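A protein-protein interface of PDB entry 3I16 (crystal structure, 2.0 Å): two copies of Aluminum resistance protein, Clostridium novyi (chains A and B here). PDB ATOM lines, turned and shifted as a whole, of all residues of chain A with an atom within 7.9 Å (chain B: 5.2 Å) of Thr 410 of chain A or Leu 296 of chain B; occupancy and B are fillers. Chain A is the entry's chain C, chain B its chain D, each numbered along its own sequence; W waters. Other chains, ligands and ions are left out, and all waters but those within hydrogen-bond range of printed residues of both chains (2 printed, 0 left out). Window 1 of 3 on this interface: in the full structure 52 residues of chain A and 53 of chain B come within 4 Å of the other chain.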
ATOM      1  N   GLY A 248     -13.240 -17.493  -8.253  1.00  0.00           N
ATOM      2  CA  GLY A 248     -13.248 -16.035  -8.116  1.00  0.00           C
ATOM      3  C   GLY A 248     -12.214 -15.488  -7.157  1.00  0.00           C
ATOM      4  O   GLY A 248     -12.426 -14.430  -6.596  1.00  0.00           O
ATOM      5  N   GLY A 249     -11.137 -16.242  -6.938  1.00  0.00           N
ATOM      6  CA  GLY A 249     -10.072 -15.849  -6.047  1.00  0.00           C
ATOM      7  C   GLY A 249     -10.305 -16.180  -4.594  1.00  0.00           C
ATOM      8  O   GLY A 249      -9.383 -16.034  -3.783  1.00  0.00           O
ATOM      9  N   ILE A 250     -11.497 -16.684  -4.247  1.00  0.00           N
ATOM     10  CA  ILE A 250     -11.799 -16.920  -2.847  1.00  0.00           C
ATOM     11  C   ILE A 250     -12.172 -18.366  -2.473  1.00  0.00           C
ATOM     12  O   ILE A 250     -12.039 -18.723  -1.330  1.00  0.00           O
ATOM     13  CB  ILE A 250     -12.806 -15.865  -2.280  1.00  0.00           C
ATOM     14  CG1 ILE A 250     -14.193 -16.054  -2.853  1.00  0.00           C
ATOM     15  CG2 ILE A 250     -12.312 -14.380  -2.518  1.00  0.00           C
ATOM     16  CD1 ILE A 250     -15.189 -15.020  -2.378  1.00  0.00           C
ATOM     17  N   LEU A 296     -18.263 -13.693  -7.985  1.00  0.00           N
ATOM     18  CA  LEU A 296     -17.151 -12.799  -8.372  1.00  0.00           C
ATOM     19  C   LEU A 296     -16.354 -13.293  -9.597  1.00  0.00           C
ATOM     20  O   LEU A 296     -15.610 -12.529 -10.196  1.00  0.00           O
ATOM     21  CB  LEU A 296     -16.171 -12.639  -7.193  1.00  0.00           C
ATOM     22  CG  LEU A 296     -16.646 -11.878  -5.952  1.00  0.00           C
ATOM     23  CD1 LEU A 296     -15.667 -12.068  -4.811  1.00  0.00           C
ATOM     24  CD2 LEU A 296     -16.843 -10.409  -6.231  1.00  0.00           C
ATOM     25  N   HIS A 299     -16.060 -11.388 -13.046  1.00  0.00           N
ATOM     26  CA  HIS A 299     -15.303 -10.174 -12.877  1.00  0.00           C
ATOM     27  C   HIS A 299     -13.821 -10.482 -12.657  1.00  0.00           C
ATOM     28  O   HIS A 299     -12.976  -9.954 -13.375  1.00  0.00           O
ATOM     29  CB  HIS A 299     -15.853  -9.392 -11.681  1.00  0.00           C
ATOM     30  CG  HIS A 299     -15.180  -8.087 -11.467  1.00  0.00           C
ATOM     31  ND1 HIS A 299     -15.631  -6.921 -12.040  1.00  0.00           N
ATOM     32  CD2 HIS A 299     -14.078  -7.759 -10.751  1.00  0.00           C
ATOM     33  CE1 HIS A 299     -14.838  -5.925 -11.678  1.00  0.00           C
ATOM     34  NE2 HIS A 299     -13.896  -6.402 -10.884  1.00  0.00           N
ATOM     35  N   ILE A 300     -13.504 -11.327 -11.674  1.00  0.00           N
ATOM     36  CA  ILE A 300     -12.088 -11.617 -11.371  1.00  0.00           C
ATOM     37  C   ILE A 300     -11.345 -12.231 -12.582  1.00  0.00           C
ATOM     38  O   ILE A 300     -10.209 -11.852 -12.850  1.00  0.00           O
ATOM     39  CB  ILE A 300     -11.898 -12.455 -10.086  1.00  0.00           C
ATOM     40  CG1 ILE A 300     -12.455 -11.693  -8.874  1.00  0.00           C
ATOM     41  CG2 ILE A 300     -10.411 -12.780  -9.834  1.00  0.00           C
ATOM     42  CD1 ILE A 300     -11.890 -10.301  -8.661  1.00  0.00           C
ATOM     43  N   MET A 302     -11.703 -11.648 -15.651  1.00  0.00           N
ATOM     44  CA  MET A 302     -11.374 -10.581 -16.574  1.00  0.00           C
ATOM     45  C   MET A 302     -10.330  -9.623 -16.024  1.00  0.00           C
ATOM     46  O   MET A 302      -9.589  -9.020 -16.793  1.00  0.00           O
ATOM     47  CB  MET A 302     -12.649  -9.875 -17.019  1.00  0.00           C
ATOM     48  CG  MET A 302     -13.540 -10.735 -17.922  1.00  0.00           C
ATOM     49  SD  MET A 302     -12.598 -11.547 -19.426  1.00  0.00           S
ATOM     50  CE  MET A 302     -14.119 -11.790 -20.623  1.00  0.00           C
ATOM     51  N   GLU A 303     -10.225  -9.501 -14.699  1.00  0.00           N
ATOM     52  CA  GLU A 303      -9.108  -8.744 -14.134  1.00  0.00           C
ATOM     53  C   GLU A 303      -7.817  -9.455 -14.545  1.00  0.00           C
ATOM     54  O   GLU A 303      -6.853  -8.819 -14.979  1.00  0.00           O
ATOM     55  CB  GLU A 303      -9.197  -8.665 -12.605  1.00  0.00           C
ATOM     56  CG  GLU A 303     -10.403  -7.880 -12.103  1.00  0.00           C
ATOM     57  CD  GLU A 303     -10.375  -6.432 -12.551  1.00  0.00           C
ATOM     58  OE1 GLU A 303      -9.332  -5.749 -12.372  1.00  0.00           O
ATOM     59  OE2 GLU A 303     -11.406  -5.970 -13.065  1.00  0.00           O
ATOM     60  N   ALA A 304      -7.804 -10.786 -14.423  1.00  0.00           N
ATOM     61  CA  ALA A 304      -6.610 -11.555 -14.803  1.00  0.00           C
ATOM     62  C   ALA A 304      -6.367 -11.467 -16.303  1.00  0.00           C
ATOM     63  O   ALA A 304      -5.225 -11.337 -16.741  1.00  0.00           O
ATOM     64  CB  ALA A 304      -6.751 -12.995 -14.388  1.00  0.00           C
ATOM     65  N   LYS A 306      -7.138  -9.077 -18.333  1.00  0.00           N
ATOM     66  CA  LYS A 306      -6.622  -7.737 -18.671  1.00  0.00           C
ATOM     67  C   LYS A 306      -5.137  -7.665 -18.369  1.00  0.00           C
ATOM     68  O   LYS A 306      -4.375  -7.086 -19.144  1.00  0.00           O
ATOM     69  CB  LYS A 306      -7.409  -6.644 -17.949  1.00  0.00           C
ATOM     70  CG  LYS A 306      -8.815  -6.453 -18.540  1.00  0.00           C
ATOM     71  CD  LYS A 306      -9.672  -5.481 -17.735  1.00  0.00           C
ATOM     72  CE  LYS A 306     -10.973  -5.163 -18.460  1.00  0.00           C
ATOM     73  NZ  LYS A 306     -11.785  -4.136 -17.748  1.00  0.00           N
ATOM     74  N   GLY A 307      -4.700  -8.309 -17.278  1.00  0.00           N
ATOM     75  CA  GLY A 307      -3.252  -8.333 -16.975  1.00  0.00           C
ATOM     76  C   GLY A 307      -2.492  -9.091 -18.069  1.00  0.00           C
ATOM     77  O   GLY A 307      -1.441  -8.647 -18.508  1.00  0.00           O
ATOM     78  N   PHE A 383      -2.894 -15.993  -1.539  1.00  0.00           N
ATOM     79  CA  PHE A 383      -3.744 -16.175  -0.376  1.00  0.00           C
ATOM     80  C   PHE A 383      -4.196 -17.636  -0.321  1.00  0.00           C
ATOM     81  O   PHE A 383      -4.272 -18.219   0.759  1.00  0.00           O
ATOM     82  CB  PHE A 383      -4.932 -15.208  -0.410  1.00  0.00           C
ATOM     83  CG  PHE A 383      -4.511 -13.770  -0.297  1.00  0.00           C
ATOM     84  CD1 PHE A 383      -4.137 -13.248   0.932  1.00  0.00           C
ATOM     85  CD2 PHE A 383      -4.395 -12.973  -1.417  1.00  0.00           C
ATOM     86  CE1 PHE A 383      -3.714 -11.923   1.041  1.00  0.00           C
ATOM     87  CE2 PHE A 383      -3.966 -11.655  -1.318  1.00  0.00           C
ATOM     88  CZ  PHE A 383      -3.628 -11.130  -0.089  1.00  0.00           C
ATOM     89  N   ILE A 389      -5.403 -18.142 -10.309  1.00  0.00           N
ATOM     90  CA  ILE A 389      -6.103 -16.885 -10.548  1.00  0.00           C
ATOM     91  C   ILE A 389      -5.414 -15.715  -9.834  1.00  0.00           C
ATOM     92  O   ILE A 389      -5.643 -14.556 -10.176  1.00  0.00           O
ATOM     93  CB  ILE A 389      -7.635 -17.003 -10.226  1.00  0.00           C
ATOM     94  CG1 ILE A 389      -8.427 -15.906 -10.938  1.00  0.00           C
ATOM     95  CG2 ILE A 389      -7.875 -16.978  -8.743  1.00  0.00           C
ATOM     96  CD1 ILE A 389      -8.204 -15.838 -12.442  1.00  0.00           C
ATOM     97  N   GLU A 390      -4.526 -16.010  -8.892  1.00  0.00           N
ATOM     98  CA  GLU A 390      -3.674 -14.973  -8.297  1.00  0.00           C
ATOM     99  C   GLU A 390      -2.393 -14.860  -9.117  1.00  0.00           C
ATOM    100  O   GLU A 390      -1.927 -15.850  -9.648  1.00  0.00           O
ATOM    101  CB  GLU A 390      -3.349 -15.321  -6.856  1.00  0.00           C
ATOM    102  CG  GLU A 390      -4.648 -15.467  -6.029  1.00  0.00           C
ATOM    103  CD  GLU A 390      -4.386 -15.658  -4.548  1.00  0.00           C
ATOM    104  OE1 GLU A 390      -3.593 -14.880  -3.984  1.00  0.00           O
ATOM    105  OE2 GLU A 390      -4.984 -16.581  -3.970  1.00  0.00           O
ATOM    106  N   LEU A 391      -1.825 -13.655  -9.204  1.00  0.00           N
ATOM    107  CA  LEU A 391      -0.646 -13.420 -10.014  1.00  0.00           C
ATOM    108  C   LEU A 391       0.448 -14.432  -9.725  1.00  0.00           C
ATOM    109  O   LEU A 391       0.859 -14.593  -8.586  1.00  0.00           O
ATOM    110  CB  LEU A 391      -0.089 -12.014  -9.791  1.00  0.00           C
ATOM    111  CG  LEU A 391       0.991 -11.574 -10.770  1.00  0.00           C
ATOM    112  CD1 LEU A 391       0.407 -11.538 -12.190  1.00  0.00           C
ATOM    113  CD2 LEU A 391       1.574 -10.200 -10.385  1.00  0.00           C
ATOM    114  N   GLY A 407      -3.029 -14.908 -13.889  1.00  0.00           N
ATOM    115  CA  GLY A 407      -3.619 -14.416 -12.657  1.00  0.00           C
ATOM    116  C   GLY A 407      -3.453 -12.934 -12.404  1.00  0.00           C
ATOM    117  O   GLY A 407      -2.743 -12.230 -13.104  1.00  0.00           O
ATOM    118  N   GLY A 408      -4.156 -12.480 -11.382  1.00  0.00           N
ATOM    119  CA  GLY A 408      -4.178 -11.094 -10.990  1.00  0.00           C
ATOM    120  C   GLY A 408      -5.578 -10.885 -10.453  1.00  0.00           C
ATOM    121  O   GLY A 408      -6.517 -10.760 -11.232  1.00  0.00           O
ATOM    122  N   LEU A 409      -5.734 -10.920  -9.126  1.00  0.00           N
ATOM    123  CA  LEU A 409      -7.052 -10.675  -8.510  1.00  0.00           C
ATOM    124  C   LEU A 409      -7.596  -9.309  -8.940  1.00  0.00           C
ATOM    125  O   LEU A 409      -8.797  -9.134  -9.014  1.00  0.00           O
ATOM    126  CB  LEU A 409      -6.996 -10.740  -6.988  1.00  0.00           C
ATOM    127  CG  LEU A 409      -6.656 -12.064  -6.336  1.00  0.00           C
ATOM    128  CD1 LEU A 409      -6.509 -11.841  -4.830  1.00  0.00           C
ATOM    129  CD2 LEU A 409      -7.698 -13.139  -6.661  1.00  0.00           C
ATOM    130  N   THR A 410      -6.710  -8.338  -9.185  1.00  0.00           N
ATOM    131  CA  THR A 410      -7.137  -7.066  -9.760  1.00  0.00           C
ATOM    132  C   THR A 410      -6.173  -6.741 -10.878  1.00  0.00           C
ATOM    133  O   THR A 410      -4.992  -7.116 -10.838  1.00  0.00           O
ATOM    134  CB  THR A 410      -7.174  -5.918  -8.746  1.00  0.00           C
ATOM    135  OG1 THR A 410      -5.836  -5.423  -8.501  1.00  0.00           O
ATOM    136  CG2 THR A 410      -7.865  -6.376  -7.448  1.00  0.00           C
ATOM    137  N   PHE A 411      -6.672  -6.062 -11.891  1.00  0.00           N
ATOM    138  CA  PHE A 411      -5.794  -5.646 -12.987  1.00  0.00           C
ATOM    139  C   PHE A 411      -4.665  -4.772 -12.465  1.00  0.00           C
ATOM    140  O   PHE A 411      -3.537  -4.898 -12.924  1.00  0.00           O
ATOM    141  CB  PHE A 411      -6.586  -4.924 -14.051  1.00  0.00           C
ATOM    142  CG  PHE A 411      -5.746  -4.292 -15.099  1.00  0.00           C
ATOM    143  CD1 PHE A 411      -4.970  -5.063 -15.935  1.00  0.00           C
ATOM    144  CD2 PHE A 411      -5.721  -2.915 -15.247  1.00  0.00           C
ATOM    145  CE1 PHE A 411      -4.200  -4.468 -16.913  1.00  0.00           C
ATOM    146  CE2 PHE A 411      -4.961  -2.329 -16.216  1.00  0.00           C
ATOM    147  CZ  PHE A 411      -4.179  -3.097 -17.040  1.00  0.00           C
ATOM    148  N   ASP A 412      -4.941  -3.891 -11.502  1.00  0.00           N
ATOM    149  CA  ASP A 412      -3.870  -3.062 -10.941  1.00  0.00           C
ATOM    150  C   ASP A 412      -2.720  -3.907 -10.357  1.00  0.00           C
ATOM    151  O   ASP A 412      -1.550  -3.536 -10.503  1.00  0.00           O
ATOM    152  CB  ASP A 412      -4.392  -2.097  -9.870  1.00  0.00           C
ATOM    153  CG  ASP A 412      -5.241  -0.967 -10.448  1.00  0.00           C
ATOM    154  OD1 ASP A 412      -4.796  -0.272 -11.398  1.00  0.00           O
ATOM    155  OD2 ASP A 412      -6.333  -0.742  -9.915  1.00  0.00           O
ATOM    156  N   HIS A 413      -3.042  -5.010  -9.679  1.00  0.00           N
ATOM    157  CA  HIS A 413      -2.005  -5.856  -9.132  1.00  0.00           C
ATOM    158  C   HIS A 413      -1.161  -6.517 -10.241  1.00  0.00           C
ATOM    159  O   HIS A 413       0.076  -6.471 -10.194  1.00  0.00           O
ATOM    160  CB  HIS A 413      -2.576  -6.893  -8.190  1.00  0.00           C
ATOM    161  CG  HIS A 413      -1.539  -7.824  -7.633  1.00  0.00           C
ATOM    162  ND1 HIS A 413      -1.752  -9.178  -7.477  1.00  0.00           N
ATOM    163  CD2 HIS A 413      -0.261  -7.600  -7.256  1.00  0.00           C
ATOM    164  CE1 HIS A 413      -0.659  -9.739  -6.991  1.00  0.00           C
ATOM    165  NE2 HIS A 413       0.262  -8.804  -6.855  1.00  0.00           N
ATOM    166  N   ALA A 414      -1.820  -7.127 -11.222  1.00  0.00           N
ATOM    167  CA  ALA A 414      -1.099  -7.748 -12.365  1.00  0.00           C
ATOM    168  C   ALA A 414      -0.198  -6.715 -13.022  1.00  0.00           C
ATOM    169  O   ALA A 414       0.968  -6.976 -13.300  1.00  0.00           O
ATOM    170  CB  ALA A 414      -2.081  -8.319 -13.383  1.00  0.00           C
ATOM    171  N   LYS A 415      -0.739  -5.519 -13.231  1.00  0.00           N
ATOM    172  CA  LYS A 415      -0.008  -4.398 -13.824  1.00  0.00           C
ATOM    173  C   LYS A 415       1.257  -4.060 -13.045  1.00  0.00           C
ATOM    174  O   LYS A 415       2.352  -3.979 -13.620  1.00  0.00           O
ATOM    175  CB  LYS A 415      -0.906  -3.162 -13.831  1.00  0.00           C
ATOM    176  CG  LYS A 415      -0.228  -1.845 -14.288  1.00  0.00           C
ATOM    177  CD  LYS A 415      -1.048  -0.620 -13.867  1.00  0.00           C
ATOM    178  CE  LYS A 415      -2.476  -0.633 -14.387  1.00  0.00           C
ATOM    179  NZ  LYS A 415      -3.265   0.439 -13.679  1.00  0.00           N
ATOM    180  N   ILE A 416       1.095  -3.858 -11.740  1.00  0.00           N
ATOM    181  CA  ILE A 416       2.226  -3.530 -10.872  1.00  0.00           C
ATOM    182  C   ILE A 416       3.335  -4.564 -10.999  1.00  0.00           C
ATOM    183  O   ILE A 416       4.490  -4.205 -11.188  1.00  0.00           O
ATOM    184  CB  ILE A 416       1.778  -3.380  -9.407  1.00  0.00           C
ATOM    185  CG1 ILE A 416       0.954  -2.090  -9.229  1.00  0.00           C
ATOM    186  CG2 ILE A 416       2.990  -3.282  -8.501  1.00  0.00           C
ATOM    187  CD1 ILE A 416       0.023  -2.086  -8.018  1.00  0.00           C
ATOM    188  N   GLN B  45      -3.949   0.439  -4.572  1.00  0.00           N
ATOM    189  CA  GLN B  45      -3.548  -0.960  -4.728  1.00  0.00           C
ATOM    190  C   GLN B  45      -2.055  -1.084  -4.412  1.00  0.00           C
ATOM    191  O   GLN B  45      -1.635  -2.026  -3.744  1.00  0.00           O
ATOM    192  CB  GLN B  45      -3.825  -1.466  -6.146  1.00  0.00           C
ATOM    193  CG  GLN B  45      -3.542  -2.957  -6.325  1.00  0.00           C
ATOM    194  CD  GLN B  45      -4.555  -3.813  -5.577  1.00  0.00           C
ATOM    195  OE1 GLN B  45      -5.627  -4.057  -6.080  1.00  0.00           O
ATOM    196  NE2 GLN B  45      -4.217  -4.242  -4.359  1.00  0.00           N
ATOM    197  N   GLY B 248     -13.115  -5.557   1.669  1.00  0.00           N
ATOM    198  CA  GLY B 248     -13.123  -5.993   0.254  1.00  0.00           C
ATOM    199  C   GLY B 248     -14.254  -6.941  -0.124  1.00  0.00           C
ATOM    200  O   GLY B 248     -14.122  -7.710  -1.060  1.00  0.00           O
ATOM    201  N   ILE B 250     -15.225  -9.525   1.556  1.00  0.00           N
ATOM    202  CA  ILE B 250     -14.977 -10.889   2.023  1.00  0.00           C
ATOM    203  C   ILE B 250     -14.621 -11.083   3.504  1.00  0.00           C
ATOM    204  O   ILE B 250     -14.746 -12.184   4.015  1.00  0.00           O
ATOM    205  CB  ILE B 250     -13.934 -11.581   1.135  1.00  0.00           C
ATOM    206  CG1 ILE B 250     -12.579 -10.920   1.227  1.00  0.00           C
ATOM    207  CG2 ILE B 250     -14.387 -11.564  -0.343  1.00  0.00           C
ATOM    208  CD1 ILE B 250     -11.505 -11.766   0.565  1.00  0.00           C
ATOM    209  N   GLN B 292      -6.899 -10.899   2.835  1.00  0.00           N
ATOM    210  CA  GLN B 292      -7.324 -10.883   1.449  1.00  0.00           C
ATOM    211  C   GLN B 292      -8.317  -9.761   1.159  1.00  0.00           C
ATOM    212  O   GLN B 292      -8.232  -9.106   0.090  1.00  0.00           O
ATOM    213  CB  GLN B 292      -7.875 -12.245   1.036  1.00  0.00           C
ATOM    214  CG  GLN B 292      -8.074 -12.360  -0.476  1.00  0.00           C
ATOM    215  CD  GLN B 292      -8.373 -13.766  -0.961  1.00  0.00           C
ATOM    216  OE1 GLN B 292      -8.559 -14.704  -0.181  1.00  0.00           O
ATOM    217  NE2 GLN B 292      -8.417 -13.914  -2.281  1.00  0.00           N
ATOM    218  N   GLY B 293      -9.258  -9.550   2.081  1.00  0.00           N
ATOM    219  CA  GLY B 293     -10.240  -8.464   1.948  1.00  0.00           C
ATOM    220  C   GLY B 293      -9.562  -7.101   1.835  1.00  0.00           C
ATOM    221  O   GLY B 293      -9.928  -6.288   0.976  1.00  0.00           O
ATOM    222  N   LEU B 294      -8.564  -6.862   2.691  1.00  0.00           N
ATOM    223  CA  LEU B 294      -7.780  -5.633   2.633  1.00  0.00           C
ATOM    224  C   LEU B 294      -7.109  -5.483   1.256  1.00  0.00           C
ATOM    225  O   LEU B 294      -7.152  -4.402   0.661  1.00  0.00           O
ATOM    226  CB  LEU B 294      -6.710  -5.624   3.744  1.00  0.00           C
ATOM    227  CG  LEU B 294      -5.708  -4.466   3.749  1.00  0.00           C
ATOM    228  CD1 LEU B 294      -6.430  -3.147   3.897  1.00  0.00           C
ATOM    229  CD2 LEU B 294      -4.625  -4.642   4.849  1.00  0.00           C
ATOM    230  N   PHE B 295      -6.519  -6.570   0.744  1.00  0.00           N
ATOM    231  CA  PHE B 295      -5.816  -6.538  -0.548  1.00  0.00           C
ATOM    232  C   PHE B 295      -6.765  -6.192  -1.700  1.00  0.00           C
ATOM    233  O   PHE B 295      -6.405  -5.439  -2.622  1.00  0.00           O
ATOM    234  CB  PHE B 295      -5.115  -7.872  -0.834  1.00  0.00           C
ATOM    235  CG  PHE B 295      -4.174  -7.810  -2.012  1.00  0.00           C
ATOM    236  CD1 PHE B 295      -2.942  -7.183  -1.886  1.00  0.00           C
ATOM    237  CD2 PHE B 295      -4.527  -8.330  -3.242  1.00  0.00           C
ATOM    238  CE1 PHE B 295      -2.064  -7.061  -2.980  1.00  0.00           C
ATOM    239  CE2 PHE B 295      -3.635  -8.243  -4.334  1.00  0.00           C
ATOM    240  CZ  PHE B 295      -2.399  -7.604  -4.185  1.00  0.00           C
ATOM    241  N   LEU B 296      -7.978  -6.732  -1.625  1.00  0.00           N
ATOM    242  CA  LEU B 296      -9.036  -6.423  -2.589  1.00  0.00           C
ATOM    243  C   LEU B 296      -9.783  -5.112  -2.350  1.00  0.00           C
ATOM    244  O   LEU B 296     -10.470  -4.650  -3.249  1.00  0.00           O
ATOM    245  CB  LEU B 296     -10.084  -7.539  -2.614  1.00  0.00           C
ATOM    246  CG  LEU B 296      -9.630  -8.866  -3.241  1.00  0.00           C
ATOM    247  CD1 LEU B 296     -10.622 -10.004  -2.894  1.00  0.00           C
ATOM    248  CD2 LEU B 296      -9.442  -8.710  -4.727  1.00  0.00           C
ATOM    249  N   ALA B 297      -9.646  -4.510  -1.176  1.00  0.00           N
ATOM    250  CA  ALA B 297     -10.450  -3.337  -0.801  1.00  0.00           C
ATOM    251  C   ALA B 297     -10.365  -2.115  -1.733  1.00  0.00           C
ATOM    252  O   ALA B 297     -11.376  -1.543  -2.066  1.00  0.00           O
ATOM    253  CB  ALA B 297     -10.186  -2.944   0.666  1.00  0.00           C
ATOM    254  N   PRO B 298      -9.167  -1.739  -2.176  1.00  0.00           N
ATOM    255  CA  PRO B 298      -9.077  -0.574  -3.047  1.00  0.00           C
ATOM    256  C   PRO B 298      -9.878  -0.751  -4.343  1.00  0.00           C
ATOM    257  O   PRO B 298     -10.490   0.206  -4.819  1.00  0.00           O
ATOM    258  CB  PRO B 298      -7.577  -0.504  -3.373  1.00  0.00           C
ATOM    259  CG  PRO B 298      -6.914  -1.042  -2.178  1.00  0.00           C
ATOM    260  CD  PRO B 298      -7.855  -2.084  -1.590  1.00  0.00           C
ATOM    261  N   HIS B 299      -9.859  -1.969  -4.889  1.00  0.00           N
ATOM    262  CA  HIS B 299     -10.588  -2.289  -6.103  1.00  0.00           C
ATOM    263  C   HIS B 299     -12.106  -2.381  -5.864  1.00  0.00           C
ATOM    264  O   HIS B 299     -12.910  -1.743  -6.563  1.00  0.00           O
ATOM    265  CB  HIS B 299     -10.048  -3.627  -6.684  1.00  0.00           C
ATOM    266  CG  HIS B 299     -10.720  -4.051  -7.946  1.00  0.00           C
ATOM    267  ND1 HIS B 299     -10.235  -3.721  -9.195  1.00  0.00           N
ATOM    268  CD2 HIS B 299     -11.818  -4.814  -8.156  1.00  0.00           C
ATOM    269  CE1 HIS B 299     -11.040  -4.225 -10.114  1.00  0.00           C
ATOM    270  NE2 HIS B 299     -12.001  -4.902  -9.512  1.00  0.00           N
ATOM    271  N   ILE B 300     -12.501  -3.176  -4.877  1.00  0.00           N
ATOM    272  CA  ILE B 300     -13.936  -3.405  -4.606  1.00  0.00           C
ATOM    273  C   ILE B 300     -14.610  -2.102  -4.184  1.00  0.00           C
ATOM    274  O   ILE B 300     -15.732  -1.828  -4.613  1.00  0.00           O
ATOM    275  CB  ILE B 300     -14.160  -4.544  -3.586  1.00  0.00           C
ATOM    276  CG1 ILE B 300     -13.595  -5.870  -4.130  1.00  0.00           C
ATOM    277  CG2 ILE B 300     -15.683  -4.759  -3.301  1.00  0.00           C
ATOM    278  CD1 ILE B 300     -14.426  -6.473  -5.263  1.00  0.00           C
ATOM    279  N   SER B 301     -13.901  -1.266  -3.418  1.00  0.00           N
ATOM    280  CA  SER B 301     -14.443   0.032  -3.007  1.00  0.00           C
ATOM    281  C   SER B 301     -14.854   0.853  -4.225  1.00  0.00           C
ATOM    282  O   SER B 301     -15.916   1.486  -4.224  1.00  0.00           O
ATOM    283  CB  SER B 301     -13.418   0.821  -2.172  1.00  0.00           C
ATOM    284  OG  SER B 301     -13.172   0.185  -0.941  1.00  0.00           O
HETATM  285  O   HOH W   1      -7.985  -2.951 -10.835  1.00  0.00           O
HETATM  286  O   HOH W   2      -7.182  -2.362  -7.972  1.00  0.00           O
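Printed residues of chain B within 4 Å of Ile 250 of chain A: Gln 292 (3.9 Å). Thr 410 of chain A touches just these residues of chain B: Gln 45, Leu 296 and His 299. Of the printed residues of chain B, Asp 412 of chain A touches Gln 45. Gly 248 of chain B touches none of the printed residues of chain A. Of the printed residues of chain A, Gln 292 of chain B touches Gly 249 (2.8 Å), Ile 250 (3.9 Å), Phe 383 (3.7 Å) and Leu 409 (3.8 Å). Of the printed residues of chain A, Phe 295 of chain B touches Phe 383 (3.7 Å) and His 413 (3.6 Å). Of chain A, only Leu 409 and Thr 410 come within 4 Å of Leu 296 of chain B. No residue of chain A comes within 4 Å of Ala 297 of chain B. The nearest residue of chain A that does not touch Leu 296 of chain B is Ile 250 of chain A (4.7 Å).
His 299 of chain B touches its own counterpart, His 299 of chain A. 5 positions are printed for both chains. Of the 14 pairs that touch across the chains among the printed residues, 1 has its exchanged pair printed and touching as well.
Water W2 lies within hydrogen-bond range of the side-chain carboxylate (OD2) of Asp 412 of chain A (2.7 Å), the side-chain amide oxygen (OE1) of Gln 45 of chain B (3.0 Å) and the side-chain hydroxyl (OG1) of Thr 410 of chain A (3.4 Å). Water W1 lies within hydrogen-bond range of ND1 of His 299 of chain B, OD2 of Asp 412 of chain A and OE1 of Glu 303 of chain A.
The side-chain amide nitrogen of Gln 45 of chain B lies within hydrogen-bond range of the backbone carbonyl oxygen of Phe 295 of chain B (3.0 Å). OE1 of Glu 390 of chain A lies within hydrogen-bond range of N of Phe 383 of chain A, 2.8 Å away. The backbone NH (N) of His 413 of chain A sits at hydrogen-bond distance from the side-chain hydroxyl (OG1) of Thr 410 of chain A (3.1 Å). The side-chain carboxylate (OE1) of Glu 303 of chain A is in hydrogen-bond range of the backbone NH (N) of Phe 411 of chain A, 2.7 Å away. OE2 of Glu 303 of chain A is in hydrogen-bond range of NE2 of His 299 of chain A, 3.3 Å away. OD1 of Asp 412 of chain A lies within salt-bridge range of NZ of Lys 415 of chain A (2.8 Å).
Among the printed residues, pairs that only touch across the chains: Ile 250 of chain A with Gln 292 of chain B (3.9 Å), Glu 303 of chain A with His 299 of chain B (3.2 Å), Phe 383 of chain A with Gln 292 of chain B (3.7 Å), Phe 383 of chain A with Phe 295 of chain B (3.7 Å), Leu 409 of chain A with Gln 292 of chain B (3.8 Å), Leu 409 of chain A with Leu 296 of chain B (3.9 Å), Thr 410 of chain A with Leu 296 of chain B (3.9 Å), Thr 410 of chain A with His 299 of chain B (3.6 Å), Asp 412 of chain A with Gln 45 of chain B (3.7 Å), His 413 of chain A with Gln 45 of chain B (3.96 Å) and His 413 of chain A with Phe 295 of chain B (3.6 Å).
The side-chain hydroxyl (OG1) of Thr 410 of chain A is in hydrogen-bond range of the side-chain amide oxygen (OE1) of Gln 45 of chain B (2.8 Å). A ring nitrogen (NE2) of His 299 of chain A is in hydrogen-bond range of a ring nitrogen (NE2) of His 299 of chain B. The side-chain amide nitrogen (NE2) of Gln 292 of chain B lies within hydrogen-bond range of the backbone carbonyl oxygen (O) of Gly 249 of chain A (2.8 Å).
Hydrophobic or aromatic side chains of chain A that line the printed part of chain B: Ile 250, His 299, Phe 383, Leu 409 and His 413.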
